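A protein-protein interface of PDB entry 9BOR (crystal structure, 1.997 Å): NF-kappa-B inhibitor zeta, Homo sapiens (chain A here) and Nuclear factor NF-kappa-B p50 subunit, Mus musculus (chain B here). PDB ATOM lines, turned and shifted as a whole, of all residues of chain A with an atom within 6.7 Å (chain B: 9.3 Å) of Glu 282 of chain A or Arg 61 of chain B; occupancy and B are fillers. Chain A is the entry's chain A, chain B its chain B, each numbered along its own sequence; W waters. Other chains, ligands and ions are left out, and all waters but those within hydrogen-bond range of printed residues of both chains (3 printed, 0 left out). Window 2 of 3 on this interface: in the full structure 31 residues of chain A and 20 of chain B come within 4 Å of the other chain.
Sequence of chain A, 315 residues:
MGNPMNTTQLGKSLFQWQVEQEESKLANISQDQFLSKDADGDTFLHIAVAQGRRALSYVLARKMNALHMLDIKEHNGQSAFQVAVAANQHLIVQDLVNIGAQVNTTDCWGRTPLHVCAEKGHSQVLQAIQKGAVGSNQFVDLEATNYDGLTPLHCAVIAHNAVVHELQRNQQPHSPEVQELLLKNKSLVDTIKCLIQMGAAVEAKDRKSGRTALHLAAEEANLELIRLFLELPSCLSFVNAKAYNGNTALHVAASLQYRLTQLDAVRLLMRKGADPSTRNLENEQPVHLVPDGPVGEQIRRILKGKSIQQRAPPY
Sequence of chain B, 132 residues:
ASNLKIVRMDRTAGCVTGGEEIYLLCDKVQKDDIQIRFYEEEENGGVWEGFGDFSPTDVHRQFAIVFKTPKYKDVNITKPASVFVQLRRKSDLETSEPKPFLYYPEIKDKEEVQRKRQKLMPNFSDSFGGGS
Of the printed residues of chain B, Asn 245 of chain A touches Thr 57. No residue of chain B comes within 4 Å of Asn 280 of chain A. Printed residues of chain B within 4 Å of Leu 281 of chain A: Arg 61. Of chain B, only Arg 61 comes within 4 Å of Glu 282 of chain A. No residue of chain B comes within 4 Å of Asn 283 of chain A. Of the printed residues of chain B, Glu 284 of chain A touches Lys 31 (3.6 Å). Gln 30 of chain B touches none of the printed residues of chain A. Printed residues of chain A within 4 Å of Lys 31 of chain B: Glu 284 (3.6 Å). Printed residues of chain A within 4 Å of Thr 57 of chain B: Asn 245 (3.7 Å). Of the printed residues of chain A, Arg 61 of chain B touches Leu 281 (3.8 Å) and Glu 282 (3.6 Å). The nearest residue of chain B that does not touch Glu 282 of chain A is Val 59 of chain B (5.2 Å).
Of the 17 printed residues of chain B, 3 touch a printed residue of chain A. Printed residues of chain A that touch a printed residue of chain B: Asn 245, Leu 281, Glu 282 and Glu 284. Hydrophobic or aromatic side chains of chain A that line the printed part of chain B: Leu 281. Among the printed residues, 4 pairs touch across the chains. Among the printed residues, Asp or Glu carboxylates within 4 Å of a Lys or Arg side-chain nitrogen of the other chain: Glu 282 of chain A with Arg 61 of chain B.
Water W2 lies within hydrogen-bond range of OE1 of Glu 282 of chain A (2.5 Å), N of Arg 61 of chain B (2.9 Å) and O of Val 59 of chain B (3.1 Å). Water W3 lies within hydrogen-bond range of the side-chain amide nitrogen of Asn 245 of chain A (2.9 Å) and the backbone carbonyl oxygen of Thr 57 of chain B (3.2 Å). Water W1 bridges the side-chain amide nitrogen (ND2) of Asn 245 of chain A (3.0 Å) and the side-chain hydroxyl (OG1) of Thr 57 of chain B (3.4 Å).
The backbone carbonyl oxygen (O) of Asn 245 of chain A sits at hydrogen-bond distance from the backbone NH (N) of Leu 281 of chain A (3.3 Å). The backbone NH (N) of Glu 282 of chain A lies within hydrogen-bond range of the side-chain amide oxygen (OD1) of Asn 280 of chain A, at 3.0 Å. The side-chain amide oxygen (OD1) of Asn 280 of chain A is in hydrogen-bond range of the backbone NH (N) of Glu 284 of chain A (2.9 Å).
Among the printed residues, pairs that only touch across the chains: Glu 284 of chain A with Lys 31 of chain B, Asn 245 of chain A with Thr 57 of chain B and Leu 281 of chain A with Arg 61 of chain B.
The guanidinium group (NE) of Arg 61 of chain B lies within salt-bridge range of the side-chain carboxylate (OE2) of Glu 282 of chain A (3.9 Å).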
ATOM      1  N   ASN A 245      -8.166 -14.844  11.506  1.00  0.00           N
ATOM      2  CA  ASN A 245      -6.842 -14.285  11.777  1.00  0.00           C
ATOM      3  C   ASN A 245      -5.739 -15.346  11.723  1.00  0.00           C
ATOM      4  O   ASN A 245      -4.588 -15.073  12.058  1.00  0.00           O
ATOM      5  CB  ASN A 245      -6.828 -13.568  13.131  1.00  0.00           C
ATOM      6  CG  ASN A 245      -7.203 -14.472  14.288  1.00  0.00           C
ATOM      7  OD1 ASN A 245      -7.216 -15.700  14.166  1.00  0.00           O
ATOM      8  ND2 ASN A 245      -7.502 -13.863  15.432  1.00  0.00           N
ATOM      9  N   GLY A 246      -6.104 -16.558  11.315  1.00  0.00           N
ATOM     10  CA  GLY A 246      -5.137 -17.628  11.127  1.00  0.00           C
ATOM     11  C   GLY A 246      -4.823 -18.438  12.372  1.00  0.00           C
ATOM     12  O   GLY A 246      -4.030 -19.375  12.327  1.00  0.00           O
ATOM     13  N   ARG A 279       1.093 -21.855  11.689  1.00  0.00           N
ATOM     14  CA  ARG A 279       1.335 -20.418  11.777  1.00  0.00           C
ATOM     15  C   ARG A 279       0.087 -19.606  11.439  1.00  0.00           C
ATOM     16  O   ARG A 279      -0.676 -19.972  10.547  1.00  0.00           O
ATOM     17  CB  ARG A 279       2.488 -20.016  10.855  1.00  0.00           C
ATOM     18  CG  ARG A 279       3.818 -20.655  11.230  1.00  0.00           C
ATOM     19  CD  ARG A 279       4.952 -20.145  10.364  1.00  0.00           C
ATOM     20  NE  ARG A 279       6.220 -20.801  10.681  1.00  0.00           N
ATOM     21  CZ  ARG A 279       7.096 -20.350  11.573  1.00  0.00           C
ATOM     22  NH1 ARG A 279       6.848 -19.231  12.245  1.00  0.00           N
ATOM     23  NH2 ARG A 279       8.228 -21.012  11.793  1.00  0.00           N
ATOM     24  N   ASN A 280      -0.120 -18.504  12.156  1.00  0.00           N
ATOM     25  CA  ASN A 280      -1.245 -17.620  11.860  1.00  0.00           C
ATOM     26  C   ASN A 280      -0.862 -16.600  10.787  1.00  0.00           C
ATOM     27  O   ASN A 280       0.216 -16.695  10.198  1.00  0.00           O
ATOM     28  CB  ASN A 280      -1.751 -16.922  13.132  1.00  0.00           C
ATOM     29  CG  ASN A 280      -0.699 -16.047  13.805  1.00  0.00           C
ATOM     30  OD1 ASN A 280       0.298 -15.653  13.199  1.00  0.00           O
ATOM     31  ND2 ASN A 280      -0.933 -15.728  15.080  1.00  0.00           N
ATOM     32  N   LEU A 281      -1.739 -15.628  10.545  1.00  0.00           N
ATOM     33  CA  LEU A 281      -1.518 -14.618   9.507  1.00  0.00           C
ATOM     34  C   LEU A 281      -0.237 -13.820   9.708  1.00  0.00           C
ATOM     35  O   LEU A 281       0.329 -13.290   8.754  1.00  0.00           O
ATOM     36  CB  LEU A 281      -2.696 -13.645   9.441  1.00  0.00           C
ATOM     37  CG  LEU A 281      -3.998 -14.164   8.840  1.00  0.00           C
ATOM     38  CD1 LEU A 281      -4.977 -13.014   8.676  1.00  0.00           C
ATOM     39  CD2 LEU A 281      -3.726 -14.852   7.510  1.00  0.00           C
ATOM     40  N   GLU A 282       0.209 -13.722  10.954  1.00  0.00           N
ATOM     41  CA  GLU A 282       1.431 -12.997  11.252  1.00  0.00           C
ATOM     42  C   GLU A 282       2.595 -13.957  11.457  1.00  0.00           C
ATOM     43  O   GLU A 282       3.591 -13.608  12.086  1.00  0.00           O
ATOM     44  CB  GLU A 282       1.231 -12.109  12.479  1.00  0.00           C
ATOM     45  CG  GLU A 282       0.189 -11.020  12.249  1.00  0.00           C
ATOM     46  CD  GLU A 282       0.122 -10.029  13.390  1.00  0.00           C
ATOM     47  OE1 GLU A 282      -0.643 -10.279  14.341  1.00  0.00           O
ATOM     48  OE2 GLU A 282       0.832  -9.003  13.339  1.00  0.00           O
ATOM     49  N   ASN A 283       2.447 -15.165  10.916  1.00  0.00           N
ATOM     50  CA  ASN A 283       3.502 -16.182  10.927  1.00  0.00           C
ATOM     51  C   ASN A 283       3.921 -16.638  12.320  1.00  0.00           C
ATOM     52  O   ASN A 283       5.021 -17.165  12.506  1.00  0.00           O
ATOM     53  CB  ASN A 283       4.728 -15.678  10.158  1.00  0.00           C
ATOM     54  CG  ASN A 283       4.518 -15.700   8.661  1.00  0.00           C
ATOM     55  OD1 ASN A 283       4.013 -16.683   8.111  1.00  0.00           O
ATOM     56  ND2 ASN A 283       4.893 -14.615   7.990  1.00  0.00           N
ATOM     57  N   GLU A 284       3.032 -16.453  13.290  1.00  0.00           N
ATOM     58  CA  GLU A 284       3.276 -16.886  14.660  1.00  0.00           C
ATOM     59  C   GLU A 284       2.804 -18.318  14.886  1.00  0.00           C
ATOM     60  O   GLU A 284       1.702 -18.702  14.466  1.00  0.00           O
ATOM     61  CB  GLU A 284       2.569 -15.955  15.655  1.00  0.00           C
ATOM     62  CG  GLU A 284       3.072 -14.517  15.653  1.00  0.00           C
ATOM     63  CD  GLU A 284       2.111 -13.563  16.361  1.00  0.00           C
ATOM     64  OE1 GLU A 284       0.880 -13.745  16.238  1.00  0.00           O
ATOM     65  OE2 GLU A 284       2.590 -12.634  17.039  1.00  0.00           O
ATOM     66  N   GLN A 285       3.642 -19.098  15.560  1.00  0.00           N
ATOM     67  CA  GLN A 285       3.256 -20.403  16.087  1.00  0.00           C
ATOM     68  C   GLN A 285       2.802 -20.233  17.533  1.00  0.00           C
ATOM     69  O   GLN A 285       3.162 -19.242  18.169  1.00  0.00           O
ATOM     70  CB  GLN A 285       4.426 -21.382  16.002  1.00  0.00           C
ATOM     71  CG  GLN A 285       4.838 -21.710  14.578  1.00  0.00           C
ATOM     72  CD  GLN A 285       6.131 -22.483  14.532  1.00  0.00           C
ATOM     73  OE1 GLN A 285       6.956 -22.380  15.440  1.00  0.00           O
ATOM     74  NE2 GLN A 285       6.311 -23.276  13.483  1.00  0.00           N
ATOM     75  N   CYS B  26      -7.834   1.562  19.326  1.00  0.00           N
ATOM     76  CA  CYS B  26      -6.890   2.273  20.175  1.00  0.00           C
ATOM     77  C   CYS B  26      -5.695   2.770  19.391  1.00  0.00           C
ATOM     78  O   CYS B  26      -5.400   2.259  18.310  1.00  0.00           O
ATOM     79  CB  CYS B  26      -6.414   1.363  21.314  1.00  0.00           C
ATOM     80  SG  CYS B  26      -5.743  -0.245  20.760  1.00  0.00           S
ATOM     81  N   ASP B  27      -4.995   3.759  19.941  1.00  0.00           N
ATOM     82  CA  ASP B  27      -3.652   4.055  19.464  1.00  0.00           C
ATOM     83  C   ASP B  27      -2.757   2.847  19.762  1.00  0.00           C
ATOM     84  O   ASP B  27      -3.176   1.912  20.439  1.00  0.00           O
ATOM     85  CB  ASP B  27      -3.097   5.328  20.107  1.00  0.00           C
ATOM     86  CG  ASP B  27      -3.669   6.596  19.489  1.00  0.00           C
ATOM     87  OD1 ASP B  27      -4.250   6.516  18.384  1.00  0.00           O
ATOM     88  OD2 ASP B  27      -3.525   7.676  20.101  1.00  0.00           O
ATOM     89  N   LYS B  28      -1.524   2.876  19.269  1.00  0.00           N
ATOM     90  CA  LYS B  28      -0.692   1.674  19.219  1.00  0.00           C
ATOM     91  C   LYS B  28      -0.389   1.082  20.594  1.00  0.00           C
ATOM     92  O   LYS B  28       0.071   1.780  21.497  1.00  0.00           O
ATOM     93  CB  LYS B  28       0.611   1.984  18.488  1.00  0.00           C
ATOM     94  CG  LYS B  28       1.289   0.772  17.870  1.00  0.00           C
ATOM     95  CD  LYS B  28       2.473   1.212  16.997  1.00  0.00           C
ATOM     96  CE  LYS B  28       3.051   0.038  16.222  1.00  0.00           C
ATOM     97  NZ  LYS B  28       4.154   0.453  15.301  1.00  0.00           N
ATOM     98  N   VAL B  29      -0.662  -0.212  20.745  1.00  0.00           N
ATOM     99  CA  VAL B  29      -0.339  -0.932  21.972  1.00  0.00           C
ATOM    100  C   VAL B  29       0.453  -2.192  21.635  1.00  0.00           C
ATOM    101  O   VAL B  29       0.534  -2.587  20.476  1.00  0.00           O
ATOM    102  CB  VAL B  29      -1.607  -1.330  22.773  1.00  0.00           C
ATOM    103  CG1 VAL B  29      -2.411  -0.091  23.158  1.00  0.00           C
ATOM    104  CG2 VAL B  29      -2.459  -2.306  21.971  1.00  0.00           C
ATOM    105  N   GLN B  30       1.048  -2.814  22.646  1.00  0.00           N
ATOM    106  CA  GLN B  30       1.719  -4.096  22.456  1.00  0.00           C
ATOM    107  C   GLN B  30       0.836  -5.158  23.096  1.00  0.00           C
ATOM    108  O   GLN B  30       0.395  -4.991  24.228  1.00  0.00           O
ATOM    109  CB  GLN B  30       3.131  -4.077  23.058  1.00  0.00           C
ATOM    110  CG  GLN B  30       4.040  -5.198  22.555  1.00  0.00           C
ATOM    111  CD  GLN B  30       3.733  -6.514  23.230  1.00  0.00           C
ATOM    112  OE1 GLN B  30       3.254  -6.536  24.366  1.00  0.00           O
ATOM    113  NE2 GLN B  30       3.995  -7.618  22.536  1.00  0.00           N
ATOM    114  N   LYS B  31       0.573  -6.240  22.368  1.00  0.00           N
ATOM    115  CA  LYS B  31      -0.487  -7.179  22.735  1.00  0.00           C
ATOM    116  C   LYS B  31      -0.324  -7.832  24.105  1.00  0.00           C
ATOM    117  O   LYS B  31      -1.317  -8.209  24.726  1.00  0.00           O
ATOM    118  CB  LYS B  31      -0.611  -8.273  21.669  1.00  0.00           C
ATOM    119  CG  LYS B  31       0.639  -9.120  21.469  1.00  0.00           C
ATOM    120  CD  LYS B  31       0.390 -10.186  20.410  1.00  0.00           C
ATOM    121  CE  LYS B  31       1.663 -10.951  20.077  1.00  0.00           C
ATOM    122  NZ  LYS B  31       2.211 -11.652  21.268  1.00  0.00           N
ATOM    123  N   PRO B  56      -3.885 -12.207  23.831  1.00  0.00           N
ATOM    124  CA  PRO B  56      -3.053 -11.400  22.929  1.00  0.00           C
ATOM    125  C   PRO B  56      -3.432 -11.514  21.450  1.00  0.00           C
ATOM    126  O   PRO B  56      -3.286 -10.532  20.720  1.00  0.00           O
ATOM    127  CB  PRO B  56      -1.649 -11.958  23.180  1.00  0.00           C
ATOM    128  CG  PRO B  56      -1.681 -12.336  24.629  1.00  0.00           C
ATOM    129  CD  PRO B  56      -3.078 -12.844  24.893  1.00  0.00           C
ATOM    130  N   THR B  57      -3.923 -12.675  21.020  1.00  0.00           N
ATOM    131  CA  THR B  57      -4.314 -12.855  19.622  1.00  0.00           C
ATOM    132  C   THR B  57      -5.557 -12.055  19.253  1.00  0.00           C
ATOM    133  O   THR B  57      -5.862 -11.892  18.075  1.00  0.00           O
ATOM    134  CB  THR B  57      -4.598 -14.330  19.282  1.00  0.00           C
ATOM    135  OG1 THR B  57      -5.577 -14.854  20.188  1.00  0.00           O
ATOM    136  CG2 THR B  57      -3.326 -15.151  19.367  1.00  0.00           C
ATOM    137  N   ASP B  58      -6.280 -11.583  20.264  1.00  0.00           N
ATOM    138  CA  ASP B  58      -7.467 -10.766  20.041  1.00  0.00           C
ATOM    139  C   ASP B  58      -7.091  -9.306  19.840  1.00  0.00           C
ATOM    140  O   ASP B  58      -7.952  -8.459  19.579  1.00  0.00           O
ATOM    141  CB  ASP B  58      -8.442 -10.895  21.211  1.00  0.00           C
ATOM    142  CG  ASP B  58      -9.037 -12.286  21.319  1.00  0.00           C
ATOM    143  OD1 ASP B  58      -9.325 -12.882  20.258  1.00  0.00           O
ATOM    144  OD2 ASP B  58      -9.205 -12.780  22.458  1.00  0.00           O
ATOM    145  N   VAL B  59      -5.805  -9.014  20.000  1.00  0.00           N
ATOM    146  CA  VAL B  59      -5.297  -7.683  19.727  1.00  0.00           C
ATOM    147  C   VAL B  59      -4.917  -7.642  18.255  1.00  0.00           C
ATOM    148  O   VAL B  59      -4.014  -8.351  17.813  1.00  0.00           O
ATOM    149  CB  VAL B  59      -4.098  -7.322  20.625  1.00  0.00           C
ATOM    150  CG1 VAL B  59      -3.581  -5.935  20.292  1.00  0.00           C
ATOM    151  CG2 VAL B  59      -4.510  -7.401  22.110  1.00  0.00           C
ATOM    152  N   HIS B  60      -5.638  -6.828  17.497  1.00  0.00           N
ATOM    153  CA  HIS B  60      -5.497  -6.789  16.050  1.00  0.00           C
ATOM    154  C   HIS B  60      -4.461  -5.758  15.620  1.00  0.00           C
ATOM    155  O   HIS B  60      -4.713  -4.555  15.669  1.00  0.00           O
ATOM    156  CB  HIS B  60      -6.848  -6.485  15.395  1.00  0.00           C
ATOM    157  CG  HIS B  60      -6.784  -6.368  13.906  1.00  0.00           C
ATOM    158  ND1 HIS B  60      -6.491  -7.436  13.086  1.00  0.00           N
ATOM    159  CD2 HIS B  60      -6.965  -5.305  13.088  1.00  0.00           C
ATOM    160  CE1 HIS B  60      -6.495  -7.036  11.827  1.00  0.00           C
ATOM    161  NE2 HIS B  60      -6.775  -5.746  11.801  1.00  0.00           N
ATOM    162  N   ARG B  61      -3.293  -6.250  15.221  1.00  0.00           N
ATOM    163  CA  ARG B  61      -2.227  -5.429  14.645  1.00  0.00           C
ATOM    164  C   ARG B  61      -1.909  -4.183  15.463  1.00  0.00           C
ATOM    165  O   ARG B  61      -1.659  -3.122  14.898  1.00  0.00           O
ATOM    166  CB  ARG B  61      -2.593  -5.014  13.220  1.00  0.00           C
ATOM    167  CG  ARG B  61      -3.053  -6.166  12.337  1.00  0.00           C
ATOM    168  CD  ARG B  61      -1.941  -7.183  12.052  1.00  0.00           C
ATOM    169  NE  ARG B  61      -2.519  -8.403  11.494  1.00  0.00           N
ATOM    170  CZ  ARG B  61      -2.727  -8.610  10.198  1.00  0.00           C
ATOM    171  NH1 ARG B  61      -2.367  -7.690   9.312  1.00  0.00           N
ATOM    172  NH2 ARG B  61      -3.287  -9.740   9.788  1.00  0.00           N
ATOM    173  N   GLN B  62      -1.944  -4.330  16.787  1.00  0.00           N
ATOM    174  CA  GLN B  62      -1.594  -3.269  17.737  1.00  0.00           C
ATOM    175  C   GLN B  62      -2.572  -2.081  17.764  1.00  0.00           C
ATOM    176  O   GLN B  62      -2.347  -1.129  18.510  1.00  0.00           O
ATOM    177  CB  GLN B  62      -0.173  -2.751  17.455  1.00  0.00           C
ATOM    178  CG  GLN B  62       0.889  -3.841  17.497  1.00  0.00           C
ATOM    179  CD  GLN B  62       2.301  -3.290  17.496  1.00  0.00           C
ATOM    180  OE1 GLN B  62       2.910  -3.137  16.441  1.00  0.00           O
ATOM    181  NE2 GLN B  62       2.830  -2.994  18.681  1.00  0.00           N
ATOM    182  N   PHE B  63      -3.660  -2.133  16.993  1.00  0.00           N
ATOM    183  CA  PHE B  63      -4.546  -0.970  16.899  1.00  0.00           C
ATOM    184  C   PHE B  63      -6.007  -1.230  17.252  1.00  0.00           C
ATOM    185  O   PHE B  63      -6.845  -0.327  17.164  1.00  0.00           O
ATOM    186  CB  PHE B  63      -4.484  -0.381  15.491  1.00  0.00           C
ATOM    187  CG  PHE B  63      -3.215   0.356  15.206  1.00  0.00           C
ATOM    188  CD1 PHE B  63      -2.922   1.531  15.877  1.00  0.00           C
ATOM    189  CD2 PHE B  63      -2.313  -0.125  14.269  1.00  0.00           C
ATOM    190  CE1 PHE B  63      -1.742   2.218  15.614  1.00  0.00           C
ATOM    191  CE2 PHE B  63      -1.137   0.561  14.004  1.00  0.00           C
ATOM    192  CZ  PHE B  63      -0.856   1.731  14.679  1.00  0.00           C
ATOM    193  N   ALA B  64      -6.326  -2.463  17.620  1.00  0.00           N
ATOM    194  CA  ALA B  64      -7.679  -2.771  18.069  1.00  0.00           C
ATOM    195  C   ALA B  64      -7.643  -3.953  19.009  1.00  0.00           C
ATOM    196  O   ALA B  64      -6.741  -4.787  18.941  1.00  0.00           O
ATOM    197  CB  ALA B  64      -8.599  -3.057  16.883  1.00  0.00           C
ATOM    198  N   ILE B  65      -8.616  -4.006  19.904  1.00  0.00           N
ATOM    199  CA  ILE B  65      -8.744  -5.112  20.836  1.00  0.00           C
ATOM    200  C   ILE B  65     -10.181  -5.586  20.842  1.00  0.00           C
ATOM    201  O   ILE B  65     -11.103  -4.789  21.014  1.00  0.00           O
ATOM    202  CB  ILE B  65      -8.336  -4.720  22.275  1.00  0.00           C
ATOM    203  CG1 ILE B  65      -6.938  -4.095  22.293  1.00  0.00           C
ATOM    204  CG2 ILE B  65      -8.411  -5.936  23.196  1.00  0.00           C
ATOM    205  CD1 ILE B  65      -6.533  -3.518  23.637  1.00  0.00           C
ATOM    206  N   VAL B  66     -10.373  -6.881  20.636  1.00  0.00           N
ATOM    207  CA  VAL B  66     -11.680  -7.485  20.822  1.00  0.00           C
ATOM    208  C   VAL B  66     -11.675  -8.210  22.159  1.00  0.00           C
ATOM    209  O   VAL B  66     -10.798  -9.035  22.416  1.00  0.00           O
ATOM    210  CB  VAL B  66     -12.024  -8.456  19.682  1.00  0.00           C
ATOM    211  CG1 VAL B  66     -13.371  -9.100  19.944  1.00  0.00           C
ATOM    212  CG2 VAL B  66     -12.020  -7.714  18.348  1.00  0.00           C
HETATM  213  O   HOH W   1      -8.002 -15.570  17.842  1.00  0.00           O
HETATM  214  O   HOH W   2      -2.724  -9.114  15.045  1.00  0.00           O
HETATM  215  O   HOH W   3      -7.567 -10.954  15.526  1.00  0.00           O
